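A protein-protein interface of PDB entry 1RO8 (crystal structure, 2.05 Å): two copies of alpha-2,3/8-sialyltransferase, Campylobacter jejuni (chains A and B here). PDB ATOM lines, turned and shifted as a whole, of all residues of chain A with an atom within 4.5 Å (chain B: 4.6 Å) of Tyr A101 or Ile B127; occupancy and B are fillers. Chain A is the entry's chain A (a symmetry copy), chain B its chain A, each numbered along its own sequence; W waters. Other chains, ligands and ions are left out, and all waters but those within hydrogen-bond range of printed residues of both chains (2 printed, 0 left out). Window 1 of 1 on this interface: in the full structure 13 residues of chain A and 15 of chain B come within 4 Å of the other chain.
ND2 of Asn B85 sits at hydrogen-bond distance from OD1 of Asp A100, 3.2 Å away.
O of Asp A100 lies close to OE1 of Gln B86.
The backbone NH of Ala B87 lies within hydrogen-bond range of the side-chain hydroxyl of Tyr A101 (3.3 Å).
The side-chain amino group (NZ) of Lys B123 is in hydrogen-bond range of the backbone carbonyl oxygen (O) of Asp A100 (2.7 Å).
The side-chain carboxylate of Glu B126 lies within salt-bridge range of the side-chain amino group of Lys A256 (3.0 Å).
O of Phe A59 is in hydrogen-bond range of OH of Tyr B128 (2.8 Å).
OD1 of Asn B130 lies within hydrogen-bond range of NZ of Lys A256, at 3.1 Å.
The backbone carbonyl oxygen (O) of His B125 lies within hydrogen-bond range of the backbone NH (N) of Asn B130 (3.1 Å).
Among the printed residues, pairs that only touch across the chains: Tyr A101 with Gln B86, Tyr A101 with Lys B123, Tyr A101 with Ile B127, Phe A102 with Tyr B128, Pro A103 with Lys B123, Ala A253 with Ile B127 and Lys A256 with Ile B127.
Printed residues of chain B within 4 Å of Tyr A101: Gln B86, Ala B87, Lys B123 and Ile B127.
Of the printed residues of chain A, Ile B127 touches Tyr A101 (3.5 Å), Ala A253 (3.5 Å) and Lys A256 (3.9 Å).
Printed residues of chain A within 4 Å of Asn B130: Lys A256.
Printed residues of chain A within 4 Å of Asn B85: Asp A100 (3.2 Å).
Of the printed residues of chain A, Lys B123 touches Asp A100, Tyr A101 and Pro A103.
Printed residues of chain B within 4 Å of Ala A253: Ile B127.
Phe A98 touches none of the printed residues of chain B.
Phe A257 touches none of the printed residues of chain B.
The nearest printed residue of chain A that does not touch Ile B127 is Phe A59 (4.02 Å).
The nearest printed residue of chain A that does not touch Asn B130 is Ala A253 (6.9 Å).
Of the 12 printed residues of chain A, 7 touch a printed residue of chain B.
Along chain A the printed residues that touch a printed residue of chain B span positions 59 to 256.
Of the 11 printed residues of chain B, 8 touch a printed residue of chain A.
Printed residues of chain B that touch a printed residue of chain A: Asn B85, Gln B86, Ala B87, Lys B123, Glu B126, Ile B127, Tyr B128 and Asn B130.
Hydrophobic or aromatic side chains of chain B that line the printed part of chain A: Ala B87, Ile B127 and Tyr B128.
Among the printed residues, 14 pairs touch across the chains.
Among the printed residues, Asp or Glu carboxylates within 4 Å of a Lys or Arg side-chain nitrogen of the other chain: Lys A256 with Glu B126 (3.0 Å).
No position is printed for both chains.
Water W1 lies within hydrogen-bond range of O of Ile B127 (2.7 Å), N of Asn B130 (3.3 Å) and NZ of Lys A256 (3.4 Å).
Water W2 lies within hydrogen-bond range of O of Tyr A101 (2.9 Å) and N of Phe B124 (3.4 Å).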
ATOM      1  N   PHE A  59     -24.535   3.892 -30.061  1.00  0.00           N
ATOM      2  CA  PHE A  59     -24.286   5.002 -29.143  1.00  0.00           C
ATOM      3  C   PHE A  59     -24.953   4.759 -27.776  1.00  0.00           C
ATOM      4  O   PHE A  59     -24.317   4.891 -26.726  1.00  0.00           O
ATOM      5  CB  PHE A  59     -24.812   6.301 -29.768  1.00  0.00           C
ATOM      6  CG  PHE A  59     -24.551   7.527 -28.939  1.00  0.00           C
ATOM      7  CD1 PHE A  59     -25.603   8.353 -28.547  1.00  0.00           C
ATOM      8  CD2 PHE A  59     -23.251   7.882 -28.586  1.00  0.00           C
ATOM      9  CE1 PHE A  59     -25.359   9.512 -27.817  1.00  0.00           C
ATOM     10  CE2 PHE A  59     -23.001   9.038 -27.858  1.00  0.00           C
ATOM     11  CZ  PHE A  59     -24.055   9.854 -27.473  1.00  0.00           C
ATOM     12  N   THR A  97     -14.838   6.851 -38.052  1.00  0.00           N
ATOM     13  CA  THR A  97     -14.253   7.344 -36.803  1.00  0.00           C
ATOM     14  C   THR A  97     -14.575   6.435 -35.621  1.00  0.00           C
ATOM     15  O   THR A  97     -14.344   6.799 -34.470  1.00  0.00           O
ATOM     16  CB  THR A  97     -14.805   8.738 -36.451  1.00  0.00           C
ATOM     17  OG1 THR A  97     -16.197   8.618 -36.128  1.00  0.00           O
ATOM     18  CG2 THR A  97     -14.643   9.699 -37.631  1.00  0.00           C
ATOM     19  N   PHE A  98     -15.106   5.255 -35.909  1.00  0.00           N
ATOM     20  CA  PHE A  98     -15.499   4.323 -34.864  1.00  0.00           C
ATOM     21  C   PHE A  98     -14.482   4.092 -33.754  1.00  0.00           C
ATOM     22  O   PHE A  98     -14.816   4.211 -32.574  1.00  0.00           O
ATOM     23  CB  PHE A  98     -15.866   2.961 -35.456  1.00  0.00           C
ATOM     24  CG  PHE A  98     -16.439   2.010 -34.441  1.00  0.00           C
ATOM     25  CD1 PHE A  98     -17.783   2.094 -34.073  1.00  0.00           C
ATOM     26  CD2 PHE A  98     -15.627   1.068 -33.810  1.00  0.00           C
ATOM     27  CE1 PHE A  98     -18.310   1.258 -33.088  1.00  0.00           C
ATOM     28  CE2 PHE A  98     -16.139   0.224 -32.824  1.00  0.00           C
ATOM     29  CZ  PHE A  98     -17.482   0.317 -32.460  1.00  0.00           C
ATOM     30  N   TYR A  99     -13.248   3.758 -34.123  1.00  0.00           N
ATOM     31  CA  TYR A  99     -12.227   3.472 -33.114  1.00  0.00           C
ATOM     32  C   TYR A  99     -11.781   4.659 -32.276  1.00  0.00           C
ATOM     33  O   TYR A  99     -11.116   4.482 -31.251  1.00  0.00           O
ATOM     34  CB  TYR A  99     -11.010   2.801 -33.761  1.00  0.00           C
ATOM     35  CG  TYR A  99     -11.319   1.412 -34.262  1.00  0.00           C
ATOM     36  CD1 TYR A  99     -11.568   1.173 -35.615  1.00  0.00           C
ATOM     37  CD2 TYR A  99     -11.420   0.345 -33.372  1.00  0.00           C
ATOM     38  CE1 TYR A  99     -11.914  -0.098 -36.069  1.00  0.00           C
ATOM     39  CE2 TYR A  99     -11.768  -0.934 -33.817  1.00  0.00           C
ATOM     40  CZ  TYR A  99     -12.016  -1.147 -35.160  1.00  0.00           C
ATOM     41  OH  TYR A  99     -12.396  -2.399 -35.585  1.00  0.00           O
ATOM     42  N   ASP A 100     -12.142   5.864 -32.709  1.00  0.00           N
ATOM     43  CA  ASP A 100     -11.793   7.072 -31.970  1.00  0.00           C
ATOM     44  C   ASP A 100     -12.876   7.435 -30.958  1.00  0.00           C
ATOM     45  O   ASP A 100     -12.613   8.137 -29.985  1.00  0.00           O
ATOM     46  CB  ASP A 100     -11.568   8.229 -32.935  1.00  0.00           C
ATOM     47  CG  ASP A 100     -10.333   8.033 -33.782  1.00  0.00           C
ATOM     48  OD1 ASP A 100     -10.387   8.388 -34.973  1.00  0.00           O
ATOM     49  OD2 ASP A 100      -9.313   7.527 -33.248  1.00  0.00           O
ATOM     50  N   TYR A 101     -14.098   6.969 -31.192  1.00  0.00           N
ATOM     51  CA  TYR A 101     -15.177   7.239 -30.248  1.00  0.00           C
ATOM     52  C   TYR A 101     -15.352   6.076 -29.273  1.00  0.00           C
ATOM     53  O   TYR A 101     -15.772   6.277 -28.138  1.00  0.00           O
ATOM     54  CB  TYR A 101     -16.500   7.514 -30.980  1.00  0.00           C
ATOM     55  CG  TYR A 101     -16.552   8.901 -31.586  1.00  0.00           C
ATOM     56  CD1 TYR A 101     -15.853   9.196 -32.750  1.00  0.00           C
ATOM     57  CD2 TYR A 101     -17.223   9.941 -30.934  1.00  0.00           C
ATOM     58  CE1 TYR A 101     -15.806  10.497 -33.257  1.00  0.00           C
ATOM     59  CE2 TYR A 101     -17.184  11.249 -31.429  1.00  0.00           C
ATOM     60  CZ  TYR A 101     -16.469  11.518 -32.589  1.00  0.00           C
ATOM     61  OH  TYR A 101     -16.387  12.799 -33.068  1.00  0.00           O
ATOM     62  N   PHE A 102     -15.025   4.863 -29.713  1.00  0.00           N
ATOM     63  CA  PHE A 102     -15.164   3.681 -28.854  1.00  0.00           C
ATOM     64  C   PHE A 102     -13.882   2.834 -28.986  1.00  0.00           C
ATOM     65  O   PHE A 102     -13.890   1.754 -29.568  1.00  0.00           O
ATOM     66  CB  PHE A 102     -16.385   2.861 -29.281  1.00  0.00           C
ATOM     67  CG  PHE A 102     -17.611   3.695 -29.580  1.00  0.00           C
ATOM     68  CD1 PHE A 102     -17.893   4.102 -30.880  1.00  0.00           C
ATOM     69  CD2 PHE A 102     -18.470   4.090 -28.561  1.00  0.00           C
ATOM     70  CE1 PHE A 102     -19.015   4.889 -31.159  1.00  0.00           C
ATOM     71  CE2 PHE A 102     -19.596   4.881 -28.834  1.00  0.00           C
ATOM     72  CZ  PHE A 102     -19.862   5.275 -30.133  1.00  0.00           C
ATOM     73  N   PRO A 103     -12.774   3.321 -28.420  1.00  0.00           N
ATOM     74  CA  PRO A 103     -11.449   2.681 -28.447  1.00  0.00           C
ATOM     75  C   PRO A 103     -11.337   1.211 -28.025  1.00  0.00           C
ATOM     76  O   PRO A 103     -10.534   0.473 -28.590  1.00  0.00           O
ATOM     77  CB  PRO A 103     -10.605   3.605 -27.565  1.00  0.00           C
ATOM     78  CG  PRO A 103     -11.265   4.945 -27.747  1.00  0.00           C
ATOM     79  CD  PRO A 103     -12.727   4.563 -27.627  1.00  0.00           C
ATOM     80  N   ALA A 253     -24.394  14.901 -24.841  1.00  0.00           N
ATOM     81  CA  ALA A 253     -23.718  13.770 -25.466  1.00  0.00           C
ATOM     82  C   ALA A 253     -24.155  13.633 -26.919  1.00  0.00           C
ATOM     83  O   ALA A 253     -23.323  13.503 -27.817  1.00  0.00           O
ATOM     84  CB  ALA A 253     -24.021  12.490 -24.701  1.00  0.00           C
ATOM     85  N   LYS A 256     -22.555  15.979 -29.274  1.00  0.00           N
ATOM     86  CA  LYS A 256     -21.177  15.651 -29.623  1.00  0.00           C
ATOM     87  C   LYS A 256     -21.093  14.513 -30.640  1.00  0.00           C
ATOM     88  O   LYS A 256     -20.166  14.461 -31.447  1.00  0.00           O
ATOM     89  CB  LYS A 256     -20.396  15.276 -28.357  1.00  0.00           C
ATOM     90  CG  LYS A 256     -20.235  16.441 -27.385  1.00  0.00           C
ATOM     91  CD  LYS A 256     -19.510  16.037 -26.110  1.00  0.00           C
ATOM     92  CE  LYS A 256     -19.272  17.254 -25.219  1.00  0.00           C
ATOM     93  NZ  LYS A 256     -18.558  16.918 -23.956  1.00  0.00           N
ATOM     94  N   PHE A 257     -22.071  13.612 -30.607  1.00  0.00           N
ATOM     95  CA  PHE A 257     -22.096  12.465 -31.512  1.00  0.00           C
ATOM     96  C   PHE A 257     -22.999  12.694 -32.730  1.00  0.00           C
ATOM     97  O   PHE A 257     -23.163  11.801 -33.565  1.00  0.00           O
ATOM     98  CB  PHE A 257     -22.576  11.229 -30.739  1.00  0.00           C
ATOM     99  CG  PHE A 257     -22.253   9.918 -31.409  1.00  0.00           C
ATOM    100  CD1 PHE A 257     -23.266   9.114 -31.922  1.00  0.00           C
ATOM    101  CD2 PHE A 257     -20.933   9.476 -31.498  1.00  0.00           C
ATOM    102  CE1 PHE A 257     -22.973   7.878 -32.513  1.00  0.00           C
ATOM    103  CE2 PHE A 257     -20.628   8.249 -32.084  1.00  0.00           C
ATOM    104  CZ  PHE A 257     -21.652   7.447 -32.591  1.00  0.00           C
ATOM    105  N   ASN A 260     -22.223  11.697 -36.366  1.00  0.00           N
ATOM    106  CA  ASN A 260     -22.313  10.270 -36.662  1.00  0.00           C
ATOM    107  C   ASN A 260     -23.764   9.808 -36.586  1.00  0.00           C
ATOM    108  O   ASN A 260     -24.041   8.610 -36.504  1.00  0.00           O
ATOM    109  CB  ASN A 260     -21.459   9.461 -35.681  1.00  0.00           C
ATOM    110  CG  ASN A 260     -20.006   9.912 -35.660  1.00  0.00           C
ATOM    111  OD1 ASN A 260     -19.408  10.170 -36.706  1.00  0.00           O
ATOM    112  ND2 ASN A 260     -19.431   9.995 -34.467  1.00  0.00           N
ATOM    113  N   ASN B  85      -8.628  13.284 -31.660  1.00  0.00           N
ATOM    114  CA  ASN B  85      -9.340  12.809 -32.837  1.00  0.00           C
ATOM    115  C   ASN B  85     -10.840  12.853 -32.556  1.00  0.00           C
ATOM    116  O   ASN B  85     -11.548  11.856 -32.699  1.00  0.00           O
ATOM    117  CB  ASN B  85      -8.909  11.386 -33.200  1.00  0.00           C
ATOM    118  CG  ASN B  85      -7.820  11.366 -34.249  1.00  0.00           C
ATOM    119  OD1 ASN B  85      -6.980  12.266 -34.300  1.00  0.00           O
ATOM    120  ND2 ASN B  85      -7.824  10.338 -35.090  1.00  0.00           N
ATOM    121  N   GLN B  86     -11.310  14.018 -32.132  1.00  0.00           N
ATOM    122  CA  GLN B  86     -12.729  14.227 -31.835  1.00  0.00           C
ATOM    123  C   GLN B  86     -13.190  15.468 -32.592  1.00  0.00           C
ATOM    124  O   GLN B  86     -12.617  16.541 -32.432  1.00  0.00           O
ATOM    125  CB  GLN B  86     -12.935  14.437 -30.338  1.00  0.00           C
ATOM    126  CG  GLN B  86     -12.687  13.200 -29.466  1.00  0.00           C
ATOM    127  CD  GLN B  86     -13.723  12.115 -29.687  1.00  0.00           C
ATOM    128  OE1 GLN B  86     -13.604  11.293 -30.598  1.00  0.00           O
ATOM    129  NE2 GLN B  86     -14.759  12.119 -28.861  1.00  0.00           N
ATOM    130  N   ALA B  87     -14.224  15.316 -33.410  1.00  0.00           N
ATOM    131  CA  ALA B  87     -14.757  16.418 -34.211  1.00  0.00           C
ATOM    132  C   ALA B  87     -15.086  17.690 -33.423  1.00  0.00           C
ATOM    133  O   ALA B  87     -14.785  18.796 -33.874  1.00  0.00           O
ATOM    134  CB  ALA B  87     -15.999  15.949 -34.976  1.00  0.00           C
ATOM    135  N   LYS B 123     -12.587   8.849 -23.544  1.00  0.00           N
ATOM    136  CA  LYS B 123     -13.685   9.056 -24.482  1.00  0.00           C
ATOM    137  C   LYS B 123     -15.054   8.883 -23.848  1.00  0.00           C
ATOM    138  O   LYS B 123     -15.962   9.681 -24.082  1.00  0.00           O
ATOM    139  CB  LYS B 123     -13.546   8.114 -25.685  1.00  0.00           C
ATOM    140  CG  LYS B 123     -12.330   8.420 -26.564  1.00  0.00           C
ATOM    141  CD  LYS B 123     -12.473   9.764 -27.288  1.00  0.00           C
ATOM    142  CE  LYS B 123     -11.139  10.250 -27.826  1.00  0.00           C
ATOM    143  NZ  LYS B 123     -10.528   9.276 -28.793  1.00  0.00           N
ATOM    144  N   PHE B 124     -15.211   7.847 -23.038  1.00  0.00           N
ATOM    145  CA  PHE B 124     -16.496   7.621 -22.403  1.00  0.00           C
ATOM    146  C   PHE B 124     -16.880   8.766 -21.462  1.00  0.00           C
ATOM    147  O   PHE B 124     -18.026   9.227 -21.472  1.00  0.00           O
ATOM    148  CB  PHE B 124     -16.490   6.298 -21.642  1.00  0.00           C
ATOM    149  CG  PHE B 124     -17.795   5.994 -20.968  1.00  0.00           C
ATOM    150  CD1 PHE B 124     -17.946   6.185 -19.603  1.00  0.00           C
ATOM    151  CD2 PHE B 124     -18.879   5.538 -21.705  1.00  0.00           C
ATOM    152  CE1 PHE B 124     -19.167   5.920 -18.979  1.00  0.00           C
ATOM    153  CE2 PHE B 124     -20.099   5.274 -21.087  1.00  0.00           C
ATOM    154  CZ  PHE B 124     -20.237   5.467 -19.723  1.00  0.00           C
ATOM    155  N   HIS B 125     -15.930   9.225 -20.652  1.00  0.00           N
ATOM    156  CA  HIS B 125     -16.212  10.314 -19.726  1.00  0.00           C
ATOM    157  C   HIS B 125     -16.414  11.652 -20.424  1.00  0.00           C
ATOM    158  O   HIS B 125     -17.288  12.431 -20.036  1.00  0.00           O
ATOM    159  CB  HIS B 125     -15.105  10.444 -18.680  1.00  0.00           C
ATOM    160  CG  HIS B 125     -15.142   9.366 -17.642  1.00  0.00           C
ATOM    161  ND1 HIS B 125     -14.630   8.103 -17.860  1.00  0.00           N
ATOM    162  CD2 HIS B 125     -15.699   9.337 -16.408  1.00  0.00           C
ATOM    163  CE1 HIS B 125     -14.875   7.344 -16.806  1.00  0.00           C
ATOM    164  NE2 HIS B 125     -15.522   8.068 -15.911  1.00  0.00           N
ATOM    165  N   GLU B 126     -15.618  11.915 -21.458  1.00  0.00           N
ATOM    166  CA  GLU B 126     -15.738  13.173 -22.179  1.00  0.00           C
ATOM    167  C   GLU B 126     -17.057  13.240 -22.939  1.00  0.00           C
ATOM    168  O   GLU B 126     -17.840  14.173 -22.764  1.00  0.00           O
ATOM    169  CB  GLU B 126     -14.576  13.352 -23.159  1.00  0.00           C
ATOM    170  CG  GLU B 126     -14.392  14.796 -23.631  1.00  0.00           C
ATOM    171  CD  GLU B 126     -15.515  15.276 -24.530  1.00  0.00           C
ATOM    172  OE1 GLU B 126     -15.708  16.508 -24.633  1.00  0.00           O
ATOM    173  OE2 GLU B 126     -16.201  14.424 -25.142  1.00  0.00           O
ATOM    174  N   ILE B 127     -17.289  12.242 -23.783  1.00  0.00           N
ATOM    175  CA  ILE B 127     -18.489  12.174 -24.600  1.00  0.00           C
ATOM    176  C   ILE B 127     -19.806  12.146 -23.827  1.00  0.00           C
ATOM    177  O   ILE B 127     -20.670  12.996 -24.038  1.00  0.00           O
ATOM    178  CB  ILE B 127     -18.443  10.942 -25.530  1.00  0.00           C
ATOM    179  CG1 ILE B 127     -17.248  11.064 -26.479  1.00  0.00           C
ATOM    180  CG2 ILE B 127     -19.746  10.819 -26.316  1.00  0.00           C
ATOM    181  CD1 ILE B 127     -17.068   9.877 -27.410  1.00  0.00           C
ATOM    182  N   TYR B 128     -19.953  11.184 -22.923  1.00  0.00           N
ATOM    183  CA  TYR B 128     -21.202  11.045 -22.196  1.00  0.00           C
ATOM    184  C   TYR B 128     -21.413  11.859 -20.928  1.00  0.00           C
ATOM    185  O   TYR B 128     -22.554  12.072 -20.526  1.00  0.00           O
ATOM    186  CB  TYR B 128     -21.453   9.570 -21.881  1.00  0.00           C
ATOM    187  CG  TYR B 128     -21.520   8.664 -23.094  1.00  0.00           C
ATOM    188  CD1 TYR B 128     -20.376   8.046 -23.594  1.00  0.00           C
ATOM    189  CD2 TYR B 128     -22.741   8.376 -23.703  1.00  0.00           C
ATOM    190  CE1 TYR B 128     -20.447   7.148 -24.663  1.00  0.00           C
ATOM    191  CE2 TYR B 128     -22.824   7.488 -24.771  1.00  0.00           C
ATOM    192  CZ  TYR B 128     -21.677   6.870 -25.244  1.00  0.00           C
ATOM    193  OH  TYR B 128     -21.776   5.936 -26.258  1.00  0.00           O
ATOM    194  N   PHE B 129     -20.342  12.315 -20.293  1.00  0.00           N
ATOM    195  CA  PHE B 129     -20.503  13.074 -19.058  1.00  0.00           C
ATOM    196  C   PHE B 129     -19.861  14.448 -19.057  1.00  0.00           C
ATOM    197  O   PHE B 129     -19.904  15.152 -18.057  1.00  0.00           O
ATOM    198  CB  PHE B 129     -19.972  12.262 -17.873  1.00  0.00           C
ATOM    199  CG  PHE B 129     -20.691  10.956 -17.668  1.00  0.00           C
ATOM    200  CD1 PHE B 129     -20.300   9.814 -18.356  1.00  0.00           C
ATOM    201  CD2 PHE B 129     -21.783  10.877 -16.805  1.00  0.00           C
ATOM    202  CE1 PHE B 129     -20.988   8.607 -18.188  1.00  0.00           C
ATOM    203  CE2 PHE B 129     -22.476   9.675 -16.632  1.00  0.00           C
ATOM    204  CZ  PHE B 129     -22.076   8.542 -17.325  1.00  0.00           C
ATOM    205  N   ASN B 130     -19.279  14.838 -20.181  1.00  0.00           N
ATOM    206  CA  ASN B 130     -18.626  16.137 -20.263  1.00  0.00           C
ATOM    207  C   ASN B 130     -17.553  16.279 -19.175  1.00  0.00           C
ATOM    208  O   ASN B 130     -17.365  17.360 -18.608  1.00  0.00           O
ATOM    209  CB  ASN B 130     -19.659  17.265 -20.133  1.00  0.00           C
ATOM    210  CG  ASN B 130     -19.078  18.624 -20.475  1.00  0.00           C
ATOM    211  OD1 ASN B 130     -18.552  18.828 -21.574  1.00  0.00           O
ATOM    212  ND2 ASN B 130     -19.168  19.563 -19.537  1.00  0.00           N
HETATM  213  O   HOH W   1     -21.292  15.265 -22.818  1.00  0.00           O
HETATM  214  O   HOH W   2     -17.118   6.653 -25.580  1.00  0.00           O
